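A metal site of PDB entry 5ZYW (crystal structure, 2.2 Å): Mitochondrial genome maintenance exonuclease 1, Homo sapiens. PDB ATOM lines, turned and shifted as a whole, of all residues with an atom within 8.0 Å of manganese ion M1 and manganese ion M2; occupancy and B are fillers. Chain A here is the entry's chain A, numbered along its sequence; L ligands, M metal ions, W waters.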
ATOM      1  N   THR A  44     -36.404  -5.561 -26.095  1.00  0.00           N
ATOM      2  CA  THR A  44     -36.431  -6.510 -24.971  1.00  0.00           C
ATOM      3  C   THR A  44     -37.831  -6.798 -24.452  1.00  0.00           C
ATOM      4  O   THR A  44     -38.095  -7.900 -23.999  1.00  0.00           O
ATOM      5  CB  THR A  44     -35.531  -6.062 -23.801  1.00  0.00           C
ATOM      6  OG1 THR A  44     -35.851  -4.716 -23.441  1.00  0.00           O
ATOM      7  CG2 THR A  44     -34.069  -6.141 -24.192  1.00  0.00           C
ATOM      8  N   GLY A  86     -24.562  -6.794 -13.813  1.00  0.00           N
ATOM      9  CA  GLY A  86     -24.877  -6.586 -15.227  1.00  0.00           C
ATOM     10  C   GLY A  86     -24.845  -5.124 -15.632  1.00  0.00           C
ATOM     11  O   GLY A  86     -24.270  -4.774 -16.658  1.00  0.00           O
ATOM     12  N   PHE A  89     -21.155  -3.560 -15.196  1.00  0.00           N
ATOM     13  CA  PHE A  89     -20.339  -4.023 -16.326  1.00  0.00           C
ATOM     14  C   PHE A  89     -20.588  -3.166 -17.574  1.00  0.00           C
ATOM     15  O   PHE A  89     -19.637  -2.767 -18.257  1.00  0.00           O
ATOM     16  CB  PHE A  89     -20.637  -5.492 -16.600  1.00  0.00           C
ATOM     17  CG  PHE A  89     -19.904  -6.057 -17.800  1.00  0.00           C
ATOM     18  CD1 PHE A  89     -18.525  -5.942 -17.903  1.00  0.00           C
ATOM     19  CD2 PHE A  89     -20.605  -6.722 -18.799  1.00  0.00           C
ATOM     20  CE1 PHE A  89     -17.859  -6.461 -19.006  1.00  0.00           C
ATOM     21  CE2 PHE A  89     -19.936  -7.249 -19.898  1.00  0.00           C
ATOM     22  CZ  PHE A  89     -18.564  -7.121 -19.992  1.00  0.00           C
ATOM     23  N   HIS A  90     -21.851  -2.873 -17.854  1.00  0.00           N
ATOM     24  CA  HIS A  90     -22.225  -2.042 -19.001  1.00  0.00           C
ATOM     25  C   HIS A  90     -21.800  -0.606 -18.860  1.00  0.00           C
ATOM     26  O   HIS A  90     -21.349  -0.010 -19.838  1.00  0.00           O
ATOM     27  CB  HIS A  90     -23.728  -2.136 -19.278  1.00  0.00           C
ATOM     28  CG  HIS A  90     -24.106  -3.381 -20.012  1.00  0.00           C
ATOM     29  ND1 HIS A  90     -24.178  -4.615 -19.398  1.00  0.00           N
ATOM     30  CD2 HIS A  90     -24.391  -3.599 -21.308  1.00  0.00           C
ATOM     31  CE1 HIS A  90     -24.503  -5.527 -20.287  1.00  0.00           C
ATOM     32  NE2 HIS A  90     -24.640  -4.931 -21.457  1.00  0.00           N
ATOM     33  N   LEU A  93     -17.941  -0.397 -19.418  1.00  0.00           N
ATOM     34  CA  LEU A  93     -17.622  -0.432 -20.858  1.00  0.00           C
ATOM     35  C   LEU A  93     -17.989   0.852 -21.603  1.00  0.00           C
ATOM     36  O   LEU A  93     -17.263   1.261 -22.495  1.00  0.00           O
ATOM     37  CB  LEU A  93     -18.287  -1.634 -21.534  1.00  0.00           C
ATOM     38  CG  LEU A  93     -17.536  -2.953 -21.382  1.00  0.00           C
ATOM     39  CD1 LEU A  93     -18.481  -4.116 -21.579  1.00  0.00           C
ATOM     40  CD2 LEU A  93     -16.372  -3.028 -22.355  1.00  0.00           C
ATOM     41  N   GLU A 133     -24.558   2.999 -26.226  1.00  0.00           N
ATOM     42  CA  GLU A 133     -25.749   3.111 -25.382  1.00  0.00           C
ATOM     43  C   GLU A 133     -26.697   4.148 -25.985  1.00  0.00           C
ATOM     44  O   GLU A 133     -27.079   5.116 -25.339  1.00  0.00           O
ATOM     45  CB  GLU A 133     -25.353   3.451 -23.939  1.00  0.00           C
ATOM     46  CG  GLU A 133     -24.621   2.315 -23.207  1.00  0.00           C
ATOM     47  CD  GLU A 133     -25.520   1.154 -22.820  1.00  0.00           C
ATOM     48  OE1 GLU A 133     -26.746   1.225 -23.063  1.00  0.00           O
ATOM     49  OE2 GLU A 133     -25.018   0.172 -22.252  1.00  0.00           O
ATOM     50  N   SER A 134     -27.029   3.921 -27.244  1.00  0.00           N
ATOM     51  CA  SER A 134     -27.674   4.912 -28.077  1.00  0.00           C
ATOM     52  C   SER A 134     -29.012   4.354 -28.537  1.00  0.00           C
ATOM     53  O   SER A 134     -29.117   3.185 -28.902  1.00  0.00           O
ATOM     54  CB  SER A 134     -26.770   5.226 -29.277  1.00  0.00           C
ATOM     55  OG  SER A 134     -27.181   6.399 -29.961  1.00  0.00           O
ATOM     56  N   GLY A 145     -35.242   0.707 -29.152  1.00  0.00           N
ATOM     57  CA  GLY A 145     -34.286  -0.021 -28.342  1.00  0.00           C
ATOM     58  C   GLY A 145     -33.033   0.768 -28.044  1.00  0.00           C
ATOM     59  O   GLY A 145     -32.845   1.859 -28.574  1.00  0.00           O
ATOM     60  N   LEU A 146     -32.198   0.210 -27.180  1.00  0.00           N
ATOM     61  CA  LEU A 146     -30.940   0.827 -26.787  1.00  0.00           C
ATOM     62  C   LEU A 146     -29.840  -0.194 -27.065  1.00  0.00           C
ATOM     63  O   LEU A 146     -29.752  -1.200 -26.377  1.00  0.00           O
ATOM     64  CB  LEU A 146     -30.995   1.215 -25.316  1.00  0.00           C
ATOM     65  CG  LEU A 146     -29.973   2.252 -24.843  1.00  0.00           C
ATOM     66  CD1 LEU A 146     -30.362   3.649 -25.317  1.00  0.00           C
ATOM     67  CD2 LEU A 146     -29.834   2.228 -23.332  1.00  0.00           C
ATOM     68  N   LEU A 147     -29.038   0.052 -28.095  1.00  0.00           N
ATOM     69  CA  LEU A 147     -27.942  -0.849 -28.433  1.00  0.00           C
ATOM     70  C   LEU A 147     -26.745  -0.486 -27.574  1.00  0.00           C
ATOM     71  O   LEU A 147     -26.580   0.670 -27.228  1.00  0.00           O
ATOM     72  CB  LEU A 147     -27.621  -0.801 -29.942  1.00  0.00           C
ATOM     73  CG  LEU A 147     -27.255   0.506 -30.691  1.00  0.00           C
ATOM     74  CD1 LEU A 147     -25.857   1.003 -30.357  1.00  0.00           C
ATOM     75  CD2 LEU A 147     -27.397   0.298 -32.187  1.00  0.00           C
ATOM     76  N   ASP A 148     -25.939  -1.482 -27.217  1.00  0.00           N
ATOM     77  CA  ASP A 148     -24.783  -1.257 -26.364  1.00  0.00           C
ATOM     78  C   ASP A 148     -23.696  -0.481 -27.081  1.00  0.00           C
ATOM     79  O   ASP A 148     -23.150   0.483 -26.526  1.00  0.00           O
ATOM     80  CB  ASP A 148     -24.165  -2.575 -25.890  1.00  0.00           C
ATOM     81  CG  ASP A 148     -24.982  -3.276 -24.828  1.00  0.00           C
ATOM     82  OD1 ASP A 148     -25.871  -2.660 -24.199  1.00  0.00           O
ATOM     83  OD2 ASP A 148     -24.697  -4.462 -24.598  1.00  0.00           O
ATOM     84  N   CYS A 149     -23.385  -0.896 -28.297  1.00  0.00           N
ATOM     85  CA  CYS A 149     -22.218  -0.373 -29.001  1.00  0.00           C
ATOM     86  C   CYS A 149     -22.232  -0.709 -30.486  1.00  0.00           C
ATOM     87  O   CYS A 149     -22.674  -1.790 -30.886  1.00  0.00           O
ATOM     88  CB  CYS A 149     -20.957  -0.940 -28.365  1.00  0.00           C
ATOM     89  SG  CYS A 149     -19.445  -0.512 -29.255  1.00  0.00           S
ATOM     90  N   ILE A 160     -22.611  -4.536 -31.442  1.00  0.00           N
ATOM     91  CA  ILE A 160     -22.104  -5.412 -30.384  1.00  0.00           C
ATOM     92  C   ILE A 160     -23.066  -5.342 -29.201  1.00  0.00           C
ATOM     93  O   ILE A 160     -23.519  -4.262 -28.840  1.00  0.00           O
ATOM     94  CB  ILE A 160     -20.712  -4.974 -29.897  1.00  0.00           C
ATOM     95  CG1 ILE A 160     -19.730  -4.908 -31.070  1.00  0.00           C
ATOM     96  CG2 ILE A 160     -20.207  -5.938 -28.807  1.00  0.00           C
ATOM     97  CD1 ILE A 160     -18.462  -4.132 -30.787  1.00  0.00           C
ATOM     98  N   ASP A 161     -23.368  -6.495 -28.608  1.00  0.00           N
ATOM     99  CA  ASP A 161     -24.059  -6.527 -27.325  1.00  0.00           C
ATOM    100  C   ASP A 161     -23.296  -7.361 -26.317  1.00  0.00           C
ATOM    101  O   ASP A 161     -23.085  -8.570 -26.500  1.00  0.00           O
ATOM    102  CB  ASP A 161     -25.509  -7.016 -27.452  1.00  0.00           C
ATOM    103  CG  ASP A 161     -26.391  -6.521 -26.311  1.00  0.00           C
ATOM    104  OD1 ASP A 161     -26.204  -6.992 -25.175  1.00  0.00           O
ATOM    105  OD2 ASP A 161     -27.252  -5.653 -26.536  1.00  0.00           O
ATOM    106  N   TRP A 162     -22.898  -6.703 -25.231  1.00  0.00           N
ATOM    107  CA  TRP A 162     -22.122  -7.315 -24.169  1.00  0.00           C
ATOM    108  C   TRP A 162     -23.103  -8.100 -23.313  1.00  0.00           C
ATOM    109  O   TRP A 162     -24.228  -7.635 -23.070  1.00  0.00           O
ATOM    110  CB  TRP A 162     -21.401  -6.247 -23.320  1.00  0.00           C
ATOM    111  CG  TRP A 162     -20.762  -5.157 -24.129  1.00  0.00           C
ATOM    112  CD1 TRP A 162     -21.226  -3.879 -24.285  1.00  0.00           C
ATOM    113  CD2 TRP A 162     -19.566  -5.244 -24.896  1.00  0.00           C
ATOM    114  NE1 TRP A 162     -20.382  -3.167 -25.111  1.00  0.00           N
ATOM    115  CE2 TRP A 162     -19.354  -3.985 -25.497  1.00  0.00           C
ATOM    116  CE3 TRP A 162     -18.636  -6.266 -25.140  1.00  0.00           C
ATOM    117  CZ2 TRP A 162     -18.257  -3.708 -26.323  1.00  0.00           C
ATOM    118  CZ3 TRP A 162     -17.537  -5.998 -25.961  1.00  0.00           C
ATOM    119  CH2 TRP A 162     -17.360  -4.731 -26.544  1.00  0.00           C
ATOM    120  N   LYS A 163     -22.690  -9.287 -22.894  1.00  0.00           N
ATOM    121  CA  LYS A 163     -23.468 -10.126 -21.988  1.00  0.00           C
ATOM    122  C   LYS A 163     -22.601 -10.619 -20.846  1.00  0.00           C
ATOM    123  O   LYS A 163     -21.414 -10.871 -21.035  1.00  0.00           O
ATOM    124  CB  LYS A 163     -24.058 -11.320 -22.749  1.00  0.00           C
ATOM    125  CG  LYS A 163     -25.028 -10.971 -23.865  1.00  0.00           C
ATOM    126  CD  LYS A 163     -26.293 -10.323 -23.346  1.00  0.00           C
ATOM    127  CE  LYS A 163     -27.223  -9.911 -24.475  1.00  0.00           C
ATOM    128  NZ  LYS A 163     -28.276  -8.974 -23.983  1.00  0.00           N
ATOM    129  N   THR A 164     -23.206 -10.729 -19.668  1.00  0.00           N
ATOM    130  CA  THR A 164     -22.579 -11.341 -18.505  1.00  0.00           C
ATOM    131  C   THR A 164     -22.980 -12.808 -18.450  1.00  0.00           C
ATOM    132  O   THR A 164     -24.149 -13.156 -18.679  1.00  0.00           O
ATOM    133  CB  THR A 164     -23.016 -10.648 -17.190  1.00  0.00           C
ATOM    134  OG1 THR A 164     -24.438 -10.532 -17.152  1.00  0.00           O
ATOM    135  CG2 THR A 164     -22.414  -9.265 -17.109  1.00  0.00           C
ATOM    136  N   PRO A 168     -28.404 -11.046 -15.983  1.00  0.00           N
ATOM    137  CA  PRO A 168     -28.858  -9.992 -15.069  1.00  0.00           C
ATOM    138  C   PRO A 168     -30.354 -10.040 -14.710  1.00  0.00           C
ATOM    139  O   PRO A 168     -30.727  -9.576 -13.621  1.00  0.00           O
ATOM    140  CB  PRO A 168     -28.529  -8.704 -15.837  1.00  0.00           C
ATOM    141  CG  PRO A 168     -28.553  -9.097 -17.265  1.00  0.00           C
ATOM    142  CD  PRO A 168     -28.070 -10.505 -17.312  1.00  0.00           C
ATOM    143  N   GLN A 173     -35.404 -13.742 -19.170  1.00  0.00           N
ATOM    144  CA  GLN A 173     -34.513 -13.623 -20.317  1.00  0.00           C
ATOM    145  C   GLN A 173     -34.085 -14.996 -20.732  1.00  0.00           C
ATOM    146  O   GLN A 173     -33.887 -15.863 -19.882  1.00  0.00           O
ATOM    147  CB  GLN A 173     -33.219 -12.890 -19.941  1.00  0.00           C
ATOM    148  CG  GLN A 173     -33.303 -11.399 -19.696  1.00  0.00           C
ATOM    149  CD  GLN A 173     -31.939 -10.830 -19.304  1.00  0.00           C
ATOM    150  OE1 GLN A 173     -31.202 -11.431 -18.496  1.00  0.00           O
ATOM    151  NE2 GLN A 173     -31.608  -9.681 -19.873  1.00  0.00           N
ATOM    152  N   ASN A 178     -30.498 -13.930 -27.700  1.00  0.00           N
ATOM    153  CA  ASN A 178     -29.500 -12.869 -27.870  1.00  0.00           C
ATOM    154  C   ASN A 178     -29.210 -12.494 -29.336  1.00  0.00           C
ATOM    155  O   ASN A 178     -29.024 -11.313 -29.636  1.00  0.00           O
ATOM    156  CB  ASN A 178     -28.200 -13.205 -27.123  1.00  0.00           C
ATOM    157  CG  ASN A 178     -28.380 -13.206 -25.603  1.00  0.00           C
ATOM    158  OD1 ASN A 178     -29.381 -12.711 -25.067  1.00  0.00           O
ATOM    159  ND2 ASN A 178     -27.401 -13.749 -24.901  1.00  0.00           N
ATOM    160  N   GLN A 181     -32.020 -10.095 -30.504  1.00  0.00           N
ATOM    161  CA  GLN A 181     -31.860  -8.746 -29.950  1.00  0.00           C
ATOM    162  C   GLN A 181     -30.884  -7.916 -30.777  1.00  0.00           C
ATOM    163  O   GLN A 181     -31.128  -6.736 -31.019  1.00  0.00           O
ATOM    164  CB  GLN A 181     -31.383  -8.808 -28.493  1.00  0.00           C
ATOM    165  CG  GLN A 181     -31.111  -7.438 -27.864  1.00  0.00           C
ATOM    166  CD  GLN A 181     -30.644  -7.531 -26.422  1.00  0.00           C
ATOM    167  OE1 GLN A 181     -30.233  -8.587 -25.935  1.00  0.00           O
ATOM    168  NE2 GLN A 181     -30.674  -6.396 -25.738  1.00  0.00           N
ATOM    169  N   TYR A 185     -31.733  -4.551 -33.226  1.00  0.00           N
ATOM    170  CA  TYR A 185     -31.067  -3.255 -33.104  1.00  0.00           C
ATOM    171  C   TYR A 185     -30.496  -2.761 -34.440  1.00  0.00           C
ATOM    172  O   TYR A 185     -30.705  -1.591 -34.807  1.00  0.00           O
ATOM    173  CB  TYR A 185     -29.943  -3.290 -32.047  1.00  0.00           C
ATOM    174  CG  TYR A 185     -30.385  -3.467 -30.593  1.00  0.00           C
ATOM    175  CD1 TYR A 185     -31.582  -2.931 -30.116  1.00  0.00           C
ATOM    176  CD2 TYR A 185     -29.569  -4.136 -29.686  1.00  0.00           C
ATOM    177  CE1 TYR A 185     -31.965  -3.078 -28.788  1.00  0.00           C
ATOM    178  CE2 TYR A 185     -29.941  -4.293 -28.360  1.00  0.00           C
ATOM    179  CZ  TYR A 185     -31.134  -3.757 -27.912  1.00  0.00           C
ATOM    180  OH  TYR A 185     -31.498  -3.914 -26.592  1.00  0.00           O
ATOM    181  N   ILE A 204     -22.133 -10.797 -30.513  1.00  0.00           N
ATOM    182  CA  ILE A 204     -22.471 -11.018 -29.101  1.00  0.00           C
ATOM    183  C   ILE A 204     -21.198 -11.395 -28.377  1.00  0.00           C
ATOM    184  O   ILE A 204     -20.450 -12.250 -28.838  1.00  0.00           O
ATOM    185  CB  ILE A 204     -23.503 -12.155 -28.927  1.00  0.00           C
ATOM    186  CG1 ILE A 204     -24.789 -11.833 -29.689  1.00  0.00           C
ATOM    187  CG2 ILE A 204     -23.795 -12.379 -27.448  1.00  0.00           C
ATOM    188  CD1 ILE A 204     -25.702 -13.027 -29.874  1.00  0.00           C
ATOM    189  N   VAL A 205     -20.956 -10.747 -27.234  1.00  0.00           N
ATOM    190  CA  VAL A 205     -19.791 -11.006 -26.403  1.00  0.00           C
ATOM    191  C   VAL A 205     -20.242 -11.453 -25.015  1.00  0.00           C
ATOM    192  O   VAL A 205     -20.905 -10.697 -24.301  1.00  0.00           O
ATOM    193  CB  VAL A 205     -18.895  -9.765 -26.278  1.00  0.00           C
ATOM    194  CG1 VAL A 205     -17.682 -10.053 -25.393  1.00  0.00           C
ATOM    195  CG2 VAL A 205     -18.461  -9.273 -27.657  1.00  0.00           C
ATOM    196  N   GLU A 254     -34.528  -1.345 -22.817  1.00  0.00           N
ATOM    197  CA  GLU A 254     -33.530  -1.473 -23.876  1.00  0.00           C
ATOM    198  C   GLU A 254     -34.041  -2.287 -25.058  1.00  0.00           C
ATOM    199  O   GLU A 254     -33.465  -2.198 -26.136  1.00  0.00           O
ATOM    200  CB  GLU A 254     -32.241  -2.069 -23.323  1.00  0.00           C
ATOM    201  CG  GLU A 254     -31.633  -1.224 -22.212  1.00  0.00           C
ATOM    202  CD  GLU A 254     -30.198  -1.599 -21.873  1.00  0.00           C
ATOM    203  OE1 GLU A 254     -29.589  -0.890 -21.045  1.00  0.00           O
ATOM    204  OE2 GLU A 254     -29.660  -2.571 -22.431  1.00  0.00           O
ATOM    205  OXT GLU A 254     -35.017  -3.028 -25.000  1.00  0.00           O
HETATM  206  O1  LIG L   1     -27.325  -4.821 -22.627  1.00  0.00           O
HETATM  207  O2  LIG L   1     -27.285  -6.927 -22.060  1.00  0.00           O
HETATM  208  C1  LIG L   1     -27.810  -5.784 -22.019  1.00  0.00           C
HETATM  209  C2  LIG L   1     -29.069  -5.589 -21.223  1.00  0.00           C
HETATM  210  O3  LIG L   1     -29.080  -6.512 -20.127  1.00  0.00           O
HETATM  211  C3  LIG L   1     -30.302  -5.775 -22.117  1.00  0.00           C
HETATM  212  O4  LIG L   1     -30.228  -6.970 -22.915  1.00  0.00           O
HETATM  213  C4  LIG L   1     -31.548  -5.790 -21.264  1.00  0.00           C
HETATM  214  O5  LIG L   1     -31.786  -4.809 -20.531  1.00  0.00           O
HETATM  215  O6  LIG L   1     -32.296  -6.794 -21.314  1.00  0.00           O
HETATM  216 MN    MN M   1     -25.502  -5.982 -23.372  1.00  0.00          MN
HETATM  217 MN    MN M   2     -27.754  -2.836 -23.359  1.00  0.00          MN
HETATM  218  O   HOH W   1     -26.983  -1.738 -21.508  1.00  0.00           O
HETATM  219  O   HOH W   2     -28.695  -3.622 -24.981  1.00  0.00           O
HETATM  220  O   HOH W   3     -28.086  -0.845 -24.092  1.00  0.00           O
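Water W2 lies within hydrogen-bond range of OD2 of Asp 161 (2.9 Å), O of Leu 146 (3.0 Å), OH of Tyr 185 (3.2 Å) and NE2 of Gln 181 (3.5 Å).
Water W1 bridges the side-chain carboxylate of Glu 254 and the side-chain carboxylate of Glu 133.
Manganese ion M2 is bound by water W2 (2.0 Å).
OD1 of Asp 148 binds manganese ion M2 (2.1 Å).
OE2 of Glu 254 is bound to manganese ion M2 (2.1 Å).
Manganese ion M2 is bound by water W3 (2.1 Å).
An oxygen (O1) of the ligand is bound to manganese ion M2 (2.2 Å).
Manganese ion M2 is bound by water W1.
The backbone carbonyl oxygen (O) of Asp 148 sits at hydrogen-bond distance from the backbone NH (N) of Glu 133, at 2.9 Å.
The backbone NH (N) of Leu 146 sits at hydrogen-bond distance from the chain-end carboxylate (O) of Glu 254 (2.9 Å).
OH of Tyr 185 is in hydrogen-bond range of O of Glu 254, at 2.6 Å.
OXT of Glu 254 sits at hydrogen-bond distance from N of Thr 44, at 3.1 Å.
OD1 of Asp 161 lies close to NZ of Lys 163 (3.1 Å).
The backbone NH (N) of Val 205 sits at hydrogen-bond distance from the backbone carbonyl oxygen (O) of Asp 161 (3.1 Å).
The backbone carbonyl oxygen (O) of Gly 86 lies within hydrogen-bond range of a ring nitrogen (ND1) of His 90 (2.7 Å).
The backbone carbonyl oxygen (O) of Leu 146 sits at hydrogen-bond distance from the side-chain hydroxyl (OH) of Tyr 185.
The backbone carbonyl oxygen (O) of Trp 162 binds manganese ion M1, at 2.1 Å.
OD2 of Asp 148 is bound to manganese ion M1, at 2.1 Å.
The side-chain carboxylate (OD1) of Asp 161 binds manganese ion M1, 2.2 Å away.
An oxygen (O1) of the ligand is bound to manganese ion M1 (2.3 Å).
Manganese ion M1 is bound by NE2 of His 90 (2.3 Å).
An oxygen (O2) of the ligand binds manganese ion M1, 2.4 Å away.
Leu 146 touches manganese ion M2 (O to MN, 3.97 Å).
Along chain A the residues within 4 Å of manganese ion M2 span positions 146 to 254.
The nearest printed residue that does not touch manganese ion M2 is His 90 (4.01 Å).
Within 4 Å of manganese ion M1: His 90, Asp 148, Asp 161 and Trp 162.
Along chain A the residues within 4 Å of manganese ion M1 span positions 90 to 162.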
